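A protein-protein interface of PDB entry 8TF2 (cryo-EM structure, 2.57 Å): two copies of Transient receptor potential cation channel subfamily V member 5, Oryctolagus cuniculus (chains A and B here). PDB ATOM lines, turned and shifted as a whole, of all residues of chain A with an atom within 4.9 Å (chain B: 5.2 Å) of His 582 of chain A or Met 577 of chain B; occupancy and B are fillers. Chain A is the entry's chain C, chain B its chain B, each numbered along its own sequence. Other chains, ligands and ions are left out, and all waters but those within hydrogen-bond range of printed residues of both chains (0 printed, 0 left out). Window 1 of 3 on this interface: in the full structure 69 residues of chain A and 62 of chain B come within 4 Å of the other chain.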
ATOM      1  N   PHE A 478      13.471  -6.511   1.850  1.00  0.00           N
ATOM      2  CA  PHE A 478      14.419  -5.478   1.440  1.00  0.00           C
ATOM      3  C   PHE A 478      15.021  -4.711   2.625  1.00  0.00           C
ATOM      4  O   PHE A 478      16.223  -4.478   2.665  1.00  0.00           O
ATOM      5  CB  PHE A 478      13.713  -4.562   0.442  1.00  0.00           C
ATOM      6  CG  PHE A 478      14.526  -3.375  -0.025  1.00  0.00           C
ATOM      7  CD1 PHE A 478      15.871  -3.529  -0.404  1.00  0.00           C
ATOM      8  CD2 PHE A 478      13.944  -2.098  -0.045  1.00  0.00           C
ATOM      9  CE1 PHE A 478      16.641  -2.408  -0.741  1.00  0.00           C
ATOM     10  CE2 PHE A 478      14.713  -0.980  -0.402  1.00  0.00           C
ATOM     11  CZ  PHE A 478      16.065  -1.132  -0.724  1.00  0.00           C
ATOM     12  N   MET A 481      17.729  -6.940   3.916  1.00  0.00           N
ATOM     13  CA  MET A 481      18.934  -6.749   3.097  1.00  0.00           C
ATOM     14  C   MET A 481      19.682  -5.484   3.468  1.00  0.00           C
ATOM     15  O   MET A 481      20.891  -5.554   3.618  1.00  0.00           O
ATOM     16  CB  MET A 481      18.661  -6.671   1.593  1.00  0.00           C
ATOM     17  CG  MET A 481      18.379  -8.011   0.938  1.00  0.00           C
ATOM     18  SD  MET A 481      19.613  -9.345   1.073  1.00  0.00           S
ATOM     19  CE  MET A 481      21.164  -8.474   0.861  1.00  0.00           C
ATOM     20  N   MET A 485      23.513  -5.853   4.703  1.00  0.00           N
ATOM     21  CA  MET A 485      24.540  -5.103   3.981  1.00  0.00           C
ATOM     22  C   MET A 485      25.247  -4.058   4.838  1.00  0.00           C
ATOM     23  O   MET A 485      26.448  -3.906   4.685  1.00  0.00           O
ATOM     24  CB  MET A 485      23.951  -4.436   2.743  1.00  0.00           C
ATOM     25  CG  MET A 485      23.466  -5.449   1.713  1.00  0.00           C
ATOM     26  SD  MET A 485      24.711  -6.572   1.053  1.00  0.00           S
ATOM     27  CE  MET A 485      23.983  -6.915  -0.551  1.00  0.00           C
ATOM     28  N   MET A 578      28.469  -6.670  -3.058  1.00  0.00           N
ATOM     29  CA  MET A 578      27.053  -6.608  -2.721  1.00  0.00           C
ATOM     30  C   MET A 578      26.209  -7.508  -3.612  1.00  0.00           C
ATOM     31  O   MET A 578      25.384  -8.248  -3.101  1.00  0.00           O
ATOM     32  CB  MET A 578      26.532  -5.187  -2.869  1.00  0.00           C
ATOM     33  CG  MET A 578      26.881  -4.306  -1.690  1.00  0.00           C
ATOM     34  SD  MET A 578      26.030  -2.734  -1.866  1.00  0.00           S
ATOM     35  CE  MET A 578      25.346  -2.576  -0.223  1.00  0.00           C
ATOM     36  N   GLY A 579      26.395  -7.484  -4.931  1.00  0.00           N
ATOM     37  CA  GLY A 579      25.689  -8.375  -5.849  1.00  0.00           C
ATOM     38  C   GLY A 579      25.931  -9.842  -5.522  1.00  0.00           C
ATOM     39  O   GLY A 579      25.006 -10.645  -5.526  1.00  0.00           O
ATOM     40  N   ASP A 580      27.157 -10.184  -5.153  1.00  0.00           N
ATOM     41  CA  ASP A 580      27.551 -11.535  -4.780  1.00  0.00           C
ATOM     42  C   ASP A 580      27.062 -11.978  -3.386  1.00  0.00           C
ATOM     43  O   ASP A 580      26.812 -13.156  -3.149  1.00  0.00           O
ATOM     44  CB  ASP A 580      29.070 -11.612  -4.895  1.00  0.00           C
ATOM     45  CG  ASP A 580      29.542 -13.049  -5.022  1.00  0.00           C
ATOM     46  OD1 ASP A 580      28.850 -13.858  -5.667  1.00  0.00           O
ATOM     47  OD2 ASP A 580      30.585 -13.398  -4.439  1.00  0.00           O
ATOM     48  N   THR A 581      26.881 -11.056  -2.449  1.00  0.00           N
ATOM     49  CA  THR A 581      26.204 -11.303  -1.173  1.00  0.00           C
ATOM     50  C   THR A 581      24.707 -11.457  -1.366  1.00  0.00           C
ATOM     51  O   THR A 581      24.100 -12.333  -0.763  1.00  0.00           O
ATOM     52  CB  THR A 581      26.466 -10.147  -0.200  1.00  0.00           C
ATOM     53  OG1 THR A 581      27.810 -10.128   0.176  1.00  0.00           O
ATOM     54  CG2 THR A 581      25.667 -10.218   1.098  1.00  0.00           C
ATOM     55  N   HIS A 582      24.097 -10.628  -2.213  1.00  0.00           N
ATOM     56  CA  HIS A 582      22.654 -10.547  -2.365  1.00  0.00           C
ATOM     57  C   HIS A 582      22.044 -11.893  -2.745  1.00  0.00           C
ATOM     58  O   HIS A 582      21.127 -12.351  -2.075  1.00  0.00           O
ATOM     59  CB  HIS A 582      22.308  -9.453  -3.385  1.00  0.00           C
ATOM     60  CG  HIS A 582      20.908  -8.927  -3.257  1.00  0.00           C
ATOM     61  ND1 HIS A 582      19.736  -9.588  -3.517  1.00  0.00           N
ATOM     62  CD2 HIS A 582      20.563  -7.712  -2.746  1.00  0.00           C
ATOM     63  CE1 HIS A 582      18.718  -8.786  -3.202  1.00  0.00           C
ATOM     64  NE2 HIS A 582      19.172  -7.634  -2.704  1.00  0.00           N
ATOM     65  N   TRP A 583      22.590 -12.581  -3.746  1.00  0.00           N
ATOM     66  CA  TRP A 583      22.033 -13.858  -4.193  1.00  0.00           C
ATOM     67  C   TRP A 583      22.179 -14.971  -3.150  1.00  0.00           C
ATOM     68  O   TRP A 583      21.314 -15.836  -3.061  1.00  0.00           O
ATOM     69  CB  TRP A 583      22.619 -14.254  -5.558  1.00  0.00           C
ATOM     70  CG  TRP A 583      24.007 -14.806  -5.601  1.00  0.00           C
ATOM     71  CD1 TRP A 583      25.111 -14.094  -5.900  1.00  0.00           C
ATOM     72  CD2 TRP A 583      24.466 -16.175  -5.403  1.00  0.00           C
ATOM     73  NE1 TRP A 583      26.220 -14.906  -5.857  1.00  0.00           N
ATOM     74  CE2 TRP A 583      25.878 -16.205  -5.586  1.00  0.00           C
ATOM     75  CE3 TRP A 583      23.837 -17.399  -5.098  1.00  0.00           C
ATOM     76  CZ2 TRP A 583      26.626 -17.382  -5.479  1.00  0.00           C
ATOM     77  CZ3 TRP A 583      24.583 -18.580  -4.946  1.00  0.00           C
ATOM     78  CH2 TRP A 583      25.973 -18.574  -5.138  1.00  0.00           C
ATOM     79  N   ARG A 584      23.228 -14.938  -2.325  1.00  0.00           N
ATOM     80  CA  ARG A 584      23.474 -15.901  -1.243  1.00  0.00           C
ATOM     81  C   ARG A 584      22.553 -15.703  -0.049  1.00  0.00           C
ATOM     82  O   ARG A 584      22.046 -16.664   0.521  1.00  0.00           O
ATOM     83  CB  ARG A 584      24.919 -15.776  -0.761  1.00  0.00           C
ATOM     84  CG  ARG A 584      25.920 -16.278  -1.794  1.00  0.00           C
ATOM     85  CD  ARG A 584      27.310 -16.272  -1.168  1.00  0.00           C
ATOM     86  NE  ARG A 584      28.270 -17.036  -1.973  1.00  0.00           N
ATOM     87  CZ  ARG A 584      28.886 -16.602  -3.040  1.00  0.00           C
ATOM     88  NH1 ARG A 584      29.742 -17.332  -3.674  1.00  0.00           N
ATOM     89  NH2 ARG A 584      28.642 -15.421  -3.489  1.00  0.00           N
ATOM     90  N   VAL A 585      22.345 -14.451   0.332  1.00  0.00           N
ATOM     91  CA  VAL A 585      21.535 -14.045   1.479  1.00  0.00           C
ATOM     92  C   VAL A 585      20.033 -14.108   1.202  1.00  0.00           C
ATOM     93  O   VAL A 585      19.263 -14.240   2.142  1.00  0.00           O
ATOM     94  CB  VAL A 585      22.000 -12.654   1.940  1.00  0.00           C
ATOM     95  CG1 VAL A 585      21.065 -11.999   2.949  1.00  0.00           C
ATOM     96  CG2 VAL A 585      23.371 -12.771   2.605  1.00  0.00           C
ATOM     97  N   ALA A 586      19.592 -14.061  -0.055  1.00  0.00           N
ATOM     98  CA  ALA A 586      18.186 -13.951  -0.435  1.00  0.00           C
ATOM     99  C   ALA A 586      17.244 -14.982   0.205  1.00  0.00           C
ATOM    100  O   ALA A 586      16.136 -14.630   0.591  1.00  0.00           O
ATOM    101  CB  ALA A 586      18.119 -14.021  -1.962  1.00  0.00           C
ATOM    102  N   ARG A 589      17.069 -13.996   3.988  1.00  0.00           N
ATOM    103  CA  ARG A 589      16.311 -12.740   4.023  1.00  0.00           C
ATOM    104  C   ARG A 589      14.799 -12.976   4.076  1.00  0.00           C
ATOM    105  O   ARG A 589      14.108 -12.320   4.846  1.00  0.00           O
ATOM    106  CB  ARG A 589      16.722 -11.951   2.779  1.00  0.00           C
ATOM    107  CG  ARG A 589      15.949 -10.659   2.527  1.00  0.00           C
ATOM    108  CD  ARG A 589      15.903 -10.341   1.034  1.00  0.00           C
ATOM    109  NE  ARG A 589      15.114 -11.311   0.265  1.00  0.00           N
ATOM    110  CZ  ARG A 589      15.215 -11.545  -1.020  1.00  0.00           C
ATOM    111  NH1 ARG A 589      14.547 -12.517  -1.539  1.00  0.00           N
ATOM    112  NH2 ARG A 589      15.970 -10.837  -1.796  1.00  0.00           N
ATOM    113  N   ASP B 489      11.336  -3.775  -7.947  1.00  0.00           N
ATOM    114  CA  ASP B 489      12.486  -3.216  -7.240  1.00  0.00           C
ATOM    115  C   ASP B 489      12.459  -1.697  -7.109  1.00  0.00           C
ATOM    116  O   ASP B 489      12.792  -1.183  -6.046  1.00  0.00           O
ATOM    117  CB  ASP B 489      13.796  -3.694  -7.878  1.00  0.00           C
ATOM    118  CG  ASP B 489      14.070  -5.176  -7.609  1.00  0.00           C
ATOM    119  OD1 ASP B 489      13.641  -5.696  -6.557  1.00  0.00           O
ATOM    120  OD2 ASP B 489      14.700  -5.825  -8.460  1.00  0.00           O
ATOM    121  N   ARG B 492       9.840  -0.752  -4.214  1.00  0.00           N
ATOM    122  CA  ARG B 492      10.399  -1.013  -2.872  1.00  0.00           C
ATOM    123  C   ARG B 492      11.471   0.018  -2.551  1.00  0.00           C
ATOM    124  O   ARG B 492      11.493   0.500  -1.437  1.00  0.00           O
ATOM    125  CB  ARG B 492      10.895  -2.459  -2.800  1.00  0.00           C
ATOM    126  CG  ARG B 492      12.212  -2.753  -3.493  1.00  0.00           C
ATOM    127  CD  ARG B 492      12.499  -4.220  -3.272  1.00  0.00           C
ATOM    128  NE  ARG B 492      11.239  -4.941  -3.248  1.00  0.00           N
ATOM    129  CZ  ARG B 492      10.783  -5.710  -4.226  1.00  0.00           C
ATOM    130  NH1 ARG B 492       9.621  -6.318  -4.099  1.00  0.00           N
ATOM    131  NH2 ARG B 492      11.497  -5.888  -5.317  1.00  0.00           N
ATOM    132  N   PHE B 493      12.337   0.316  -3.490  1.00  0.00           N
ATOM    133  CA  PHE B 493      13.400   1.283  -3.299  1.00  0.00           C
ATOM    134  C   PHE B 493      12.858   2.680  -3.023  1.00  0.00           C
ATOM    135  O   PHE B 493      13.226   3.272  -2.017  1.00  0.00           O
ATOM    136  CB  PHE B 493      14.335   1.281  -4.502  1.00  0.00           C
ATOM    137  CG  PHE B 493      15.619   2.003  -4.205  1.00  0.00           C
ATOM    138  CD1 PHE B 493      16.585   1.364  -3.416  1.00  0.00           C
ATOM    139  CD2 PHE B 493      15.840   3.310  -4.666  1.00  0.00           C
ATOM    140  CE1 PHE B 493      17.774   2.023  -3.094  1.00  0.00           C
ATOM    141  CE2 PHE B 493      17.042   3.963  -4.361  1.00  0.00           C
ATOM    142  CZ  PHE B 493      18.013   3.313  -3.586  1.00  0.00           C
ATOM    143  N   LEU B 573      23.176  -0.857  -3.536  1.00  0.00           N
ATOM    144  CA  LEU B 573      22.289  -1.960  -3.197  1.00  0.00           C
ATOM    145  C   LEU B 573      21.102  -2.066  -4.162  1.00  0.00           C
ATOM    146  O   LEU B 573      20.657  -3.168  -4.451  1.00  0.00           O
ATOM    147  CB  LEU B 573      21.850  -1.793  -1.737  1.00  0.00           C
ATOM    148  CG  LEU B 573      20.931  -2.899  -1.203  1.00  0.00           C
ATOM    149  CD1 LEU B 573      21.540  -4.284  -1.390  1.00  0.00           C
ATOM    150  CD2 LEU B 573      20.682  -2.662   0.283  1.00  0.00           C
ATOM    151  N   PHE B 574      20.626  -0.963  -4.738  1.00  0.00           N
ATOM    152  CA  PHE B 574      19.638  -0.995  -5.811  1.00  0.00           C
ATOM    153  C   PHE B 574      20.142  -1.770  -7.033  1.00  0.00           C
ATOM    154  O   PHE B 574      19.467  -2.674  -7.508  1.00  0.00           O
ATOM    155  CB  PHE B 574      19.226   0.431  -6.186  1.00  0.00           C
ATOM    156  CG  PHE B 574      18.084   0.493  -7.171  1.00  0.00           C
ATOM    157  CD1 PHE B 574      16.823   0.023  -6.787  1.00  0.00           C
ATOM    158  CD2 PHE B 574      18.269   0.981  -8.471  1.00  0.00           C
ATOM    159  CE1 PHE B 574      15.752   0.039  -7.686  1.00  0.00           C
ATOM    160  CE2 PHE B 574      17.190   1.009  -9.370  1.00  0.00           C
ATOM    161  CZ  PHE B 574      15.928   0.547  -8.977  1.00  0.00           C
ATOM    162  N   ILE B 575      21.366  -1.491  -7.490  1.00  0.00           N
ATOM    163  CA  ILE B 575      22.023  -2.235  -8.570  1.00  0.00           C
ATOM    164  C   ILE B 575      22.132  -3.715  -8.209  1.00  0.00           C
ATOM    165  O   ILE B 575      21.801  -4.569  -9.023  1.00  0.00           O
ATOM    166  CB  ILE B 575      23.426  -1.675  -8.902  1.00  0.00           C
ATOM    167  CG1 ILE B 575      23.450  -0.157  -9.161  1.00  0.00           C
ATOM    168  CG2 ILE B 575      23.990  -2.417 -10.125  1.00  0.00           C
ATOM    169  CD1 ILE B 575      24.845   0.458  -9.074  1.00  0.00           C
ATOM    170  N   ALA B 576      22.559  -4.038  -6.989  1.00  0.00           N
ATOM    171  CA  ALA B 576      22.685  -5.408  -6.522  1.00  0.00           C
ATOM    172  C   ALA B 576      21.344  -6.151  -6.519  1.00  0.00           C
ATOM    173  O   ALA B 576      21.268  -7.253  -7.054  1.00  0.00           O
ATOM    174  CB  ALA B 576      23.341  -5.400  -5.146  1.00  0.00           C
ATOM    175  N   MET B 577      20.271  -5.566  -5.988  1.00  0.00           N
ATOM    176  CA  MET B 577      18.977  -6.239  -5.972  1.00  0.00           C
ATOM    177  C   MET B 577      18.340  -6.330  -7.353  1.00  0.00           C
ATOM    178  O   MET B 577      17.758  -7.359  -7.671  1.00  0.00           O
ATOM    179  CB  MET B 577      18.040  -5.653  -4.921  1.00  0.00           C
ATOM    180  CG  MET B 577      17.275  -4.388  -5.269  1.00  0.00           C
ATOM    181  SD  MET B 577      15.920  -4.143  -4.102  1.00  0.00           S
ATOM    182  CE  MET B 577      15.679  -2.375  -4.280  1.00  0.00           C
ATOM    183  N   MET B 578      18.531  -5.338  -8.223  1.00  0.00           N
ATOM    184  CA  MET B 578      18.176  -5.455  -9.631  1.00  0.00           C
ATOM    185  C   MET B 578      18.932  -6.579 -10.324  1.00  0.00           C
ATOM    186  O   MET B 578      18.316  -7.368 -11.023  1.00  0.00           O
ATOM    187  CB  MET B 578      18.488  -4.162 -10.368  1.00  0.00           C
ATOM    188  CG  MET B 578      17.434  -3.096 -10.161  1.00  0.00           C
ATOM    189  SD  MET B 578      17.786  -1.710 -11.248  1.00  0.00           S
ATOM    190  CE  MET B 578      16.161  -1.455 -11.946  1.00  0.00           C
ATOM    191  N   GLY B 579      20.247  -6.692 -10.146  1.00  0.00           N
ATOM    192  CA  GLY B 579      21.033  -7.791 -10.703  1.00  0.00           C
ATOM    193  C   GLY B 579      20.531  -9.150 -10.235  1.00  0.00           C
ATOM    194  O   GLY B 579      20.417 -10.079 -11.023  1.00  0.00           O
ATOM    195  N   ASP B 580      20.147  -9.249  -8.971  1.00  0.00           N
ATOM    196  CA  ASP B 580      19.618 -10.464  -8.370  1.00  0.00           C
ATOM    197  C   ASP B 580      18.171 -10.799  -8.783  1.00  0.00           C
ATOM    198  O   ASP B 580      17.785 -11.962  -8.846  1.00  0.00           O
ATOM    199  CB  ASP B 580      19.753 -10.319  -6.857  1.00  0.00           C
ATOM    200  CG  ASP B 580      19.710 -11.669  -6.166  1.00  0.00           C
ATOM    201  OD1 ASP B 580      20.237 -12.650  -6.724  1.00  0.00           O
ATOM    202  OD2 ASP B 580      19.110 -11.776  -5.082  1.00  0.00           O
ATOM    203  N   THR B 581      17.352  -9.806  -9.105  1.00  0.00           N
ATOM    204  CA  THR B 581      16.042  -9.993  -9.735  1.00  0.00           C
ATOM    205  C   THR B 581      16.185 -10.400 -11.190  1.00  0.00           C
ATOM    206  O   THR B 581      15.466 -11.277 -11.652  1.00  0.00           O
ATOM    207  CB  THR B 581      15.225  -8.698  -9.657  1.00  0.00           C
ATOM    208  OG1 THR B 581      14.881  -8.423  -8.332  1.00  0.00           O
ATOM    209  CG2 THR B 581      13.913  -8.728 -10.434  1.00  0.00           C
ATOM    210  N   HIS B 582      17.115  -9.788 -11.923  1.00  0.00           N
ATOM    211  CA  HIS B 582      17.247  -9.952 -13.361  1.00  0.00           C
ATOM    212  C   HIS B 582      17.445 -11.413 -13.753  1.00  0.00           C
ATOM    213  O   HIS B 582      16.706 -11.920 -14.586  1.00  0.00           O
ATOM    214  CB  HIS B 582      18.388  -9.062 -13.873  1.00  0.00           C
ATOM    215  CG  HIS B 582      18.298  -8.747 -15.338  1.00  0.00           C
ATOM    216  ND1 HIS B 582      18.452  -9.610 -16.392  1.00  0.00           N
ATOM    217  CD2 HIS B 582      17.935  -7.546 -15.869  1.00  0.00           C
ATOM    218  CE1 HIS B 582      18.217  -8.942 -17.522  1.00  0.00           C
ATOM    219  NE2 HIS B 582      17.875  -7.680 -17.254  1.00  0.00           N
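A ring nitrogen (ND1) of His 582 of chain A sits at hydrogen-bond distance from the side-chain carboxylate (OD2) of Asp 580 of chain B, 2.8 Å away.
The backbone carbonyl oxygen of Met 577 of chain B sits at hydrogen-bond distance from the side-chain hydroxyl of Thr 581 of chain B, at 3.1 Å.
The side-chain carboxylate (OD1) of Asp 580 of chain A sits at hydrogen-bond distance from the indole nitrogen (NE1) of Trp 583 of chain A.
The guanidinium group (NH1) of Arg 589 of chain A lies within hydrogen-bond range of the backbone carbonyl oxygen (O) of Ala 586 of chain A.
The side-chain carboxylate of Asp 489 of chain B is in salt-bridge range of the guanidinium group of Arg 492 of chain B, 2.5 Å away.
Arg 492 of chain B touches Phe 478 of chain A (O to CE2, 3.7 Å).
CE1 of Phe 478 of chain A touches CE of Met 577 of chain B (3.7 Å).
CD1 of Leu 573 of chain B touches CE of Met 485 of chain A, 3.7 Å away.
Met 578 of chain A touches Leu 573 of chain B (SD to N, 3.8 Å).
Met 578 of chain A touches Ala 576 of chain B (C to CB, 3.9 Å).
Ala 576 of chain B touches Gly 579 of chain A.
CD2 of His 582 of chain A touches CD1 of Leu 573 of chain B (3.8 Å).
His 582 of chain A touches Met 577 of chain B (NE2 to CB, 3.2 Å).
CB of Trp 583 of chain A touches OD1 of Asp 580 of chain B, at 3.1 Å.
Ala 586 of chain A touches Asp 580 of chain B (CB to OD2, 3.97 Å).
Of the printed residues of chain B, Met 485 of chain A touches Leu 573.
Of the printed residues of chain B, His 582 of chain A touches Leu 573, Met 577 and Asp 580.
Of the printed residues of chain B, Ala 586 of chain A touches Asp 580 (3.97 Å).
Of the printed residues of chain A, Arg 492 of chain B touches Phe 478 (3.7 Å).
Printed residues of chain A within 4 Å of Phe 493 of chain B: Phe 478 (3.7 Å).
Ile 575 of chain B touches none of the printed residues of chain A.
The nearest residue of chain B that does not touch His 582 of chain A is Ala 576 of chain B (4.2 Å).
Hydrophobic or aromatic side chains of chain B that line the printed part of chain A: Phe 493, Leu 573, Ala 576 and Met 577.
Of the 13 printed residues of chain A, 7 touch a printed residue of chain B.
Printed residues of chain A that touch a printed residue of chain B: Phe 478, Met 485, Met 578, Gly 579, His 582, Trp 583 and Ala 586.
Among the printed residues, 12 pairs touch across the chains.
His 582 of chain A touches Asp 580 of chain B, but with the chains exchanged Asp 580 of chain A does not touch His 582 of chain B (12.1 Å).
Positions printed for both chains: 578, 579, 580, 581 and 582.
Of the 12 pairs that touch across the chains among the printed residues, none has its exchanged pair printed and touching as well.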
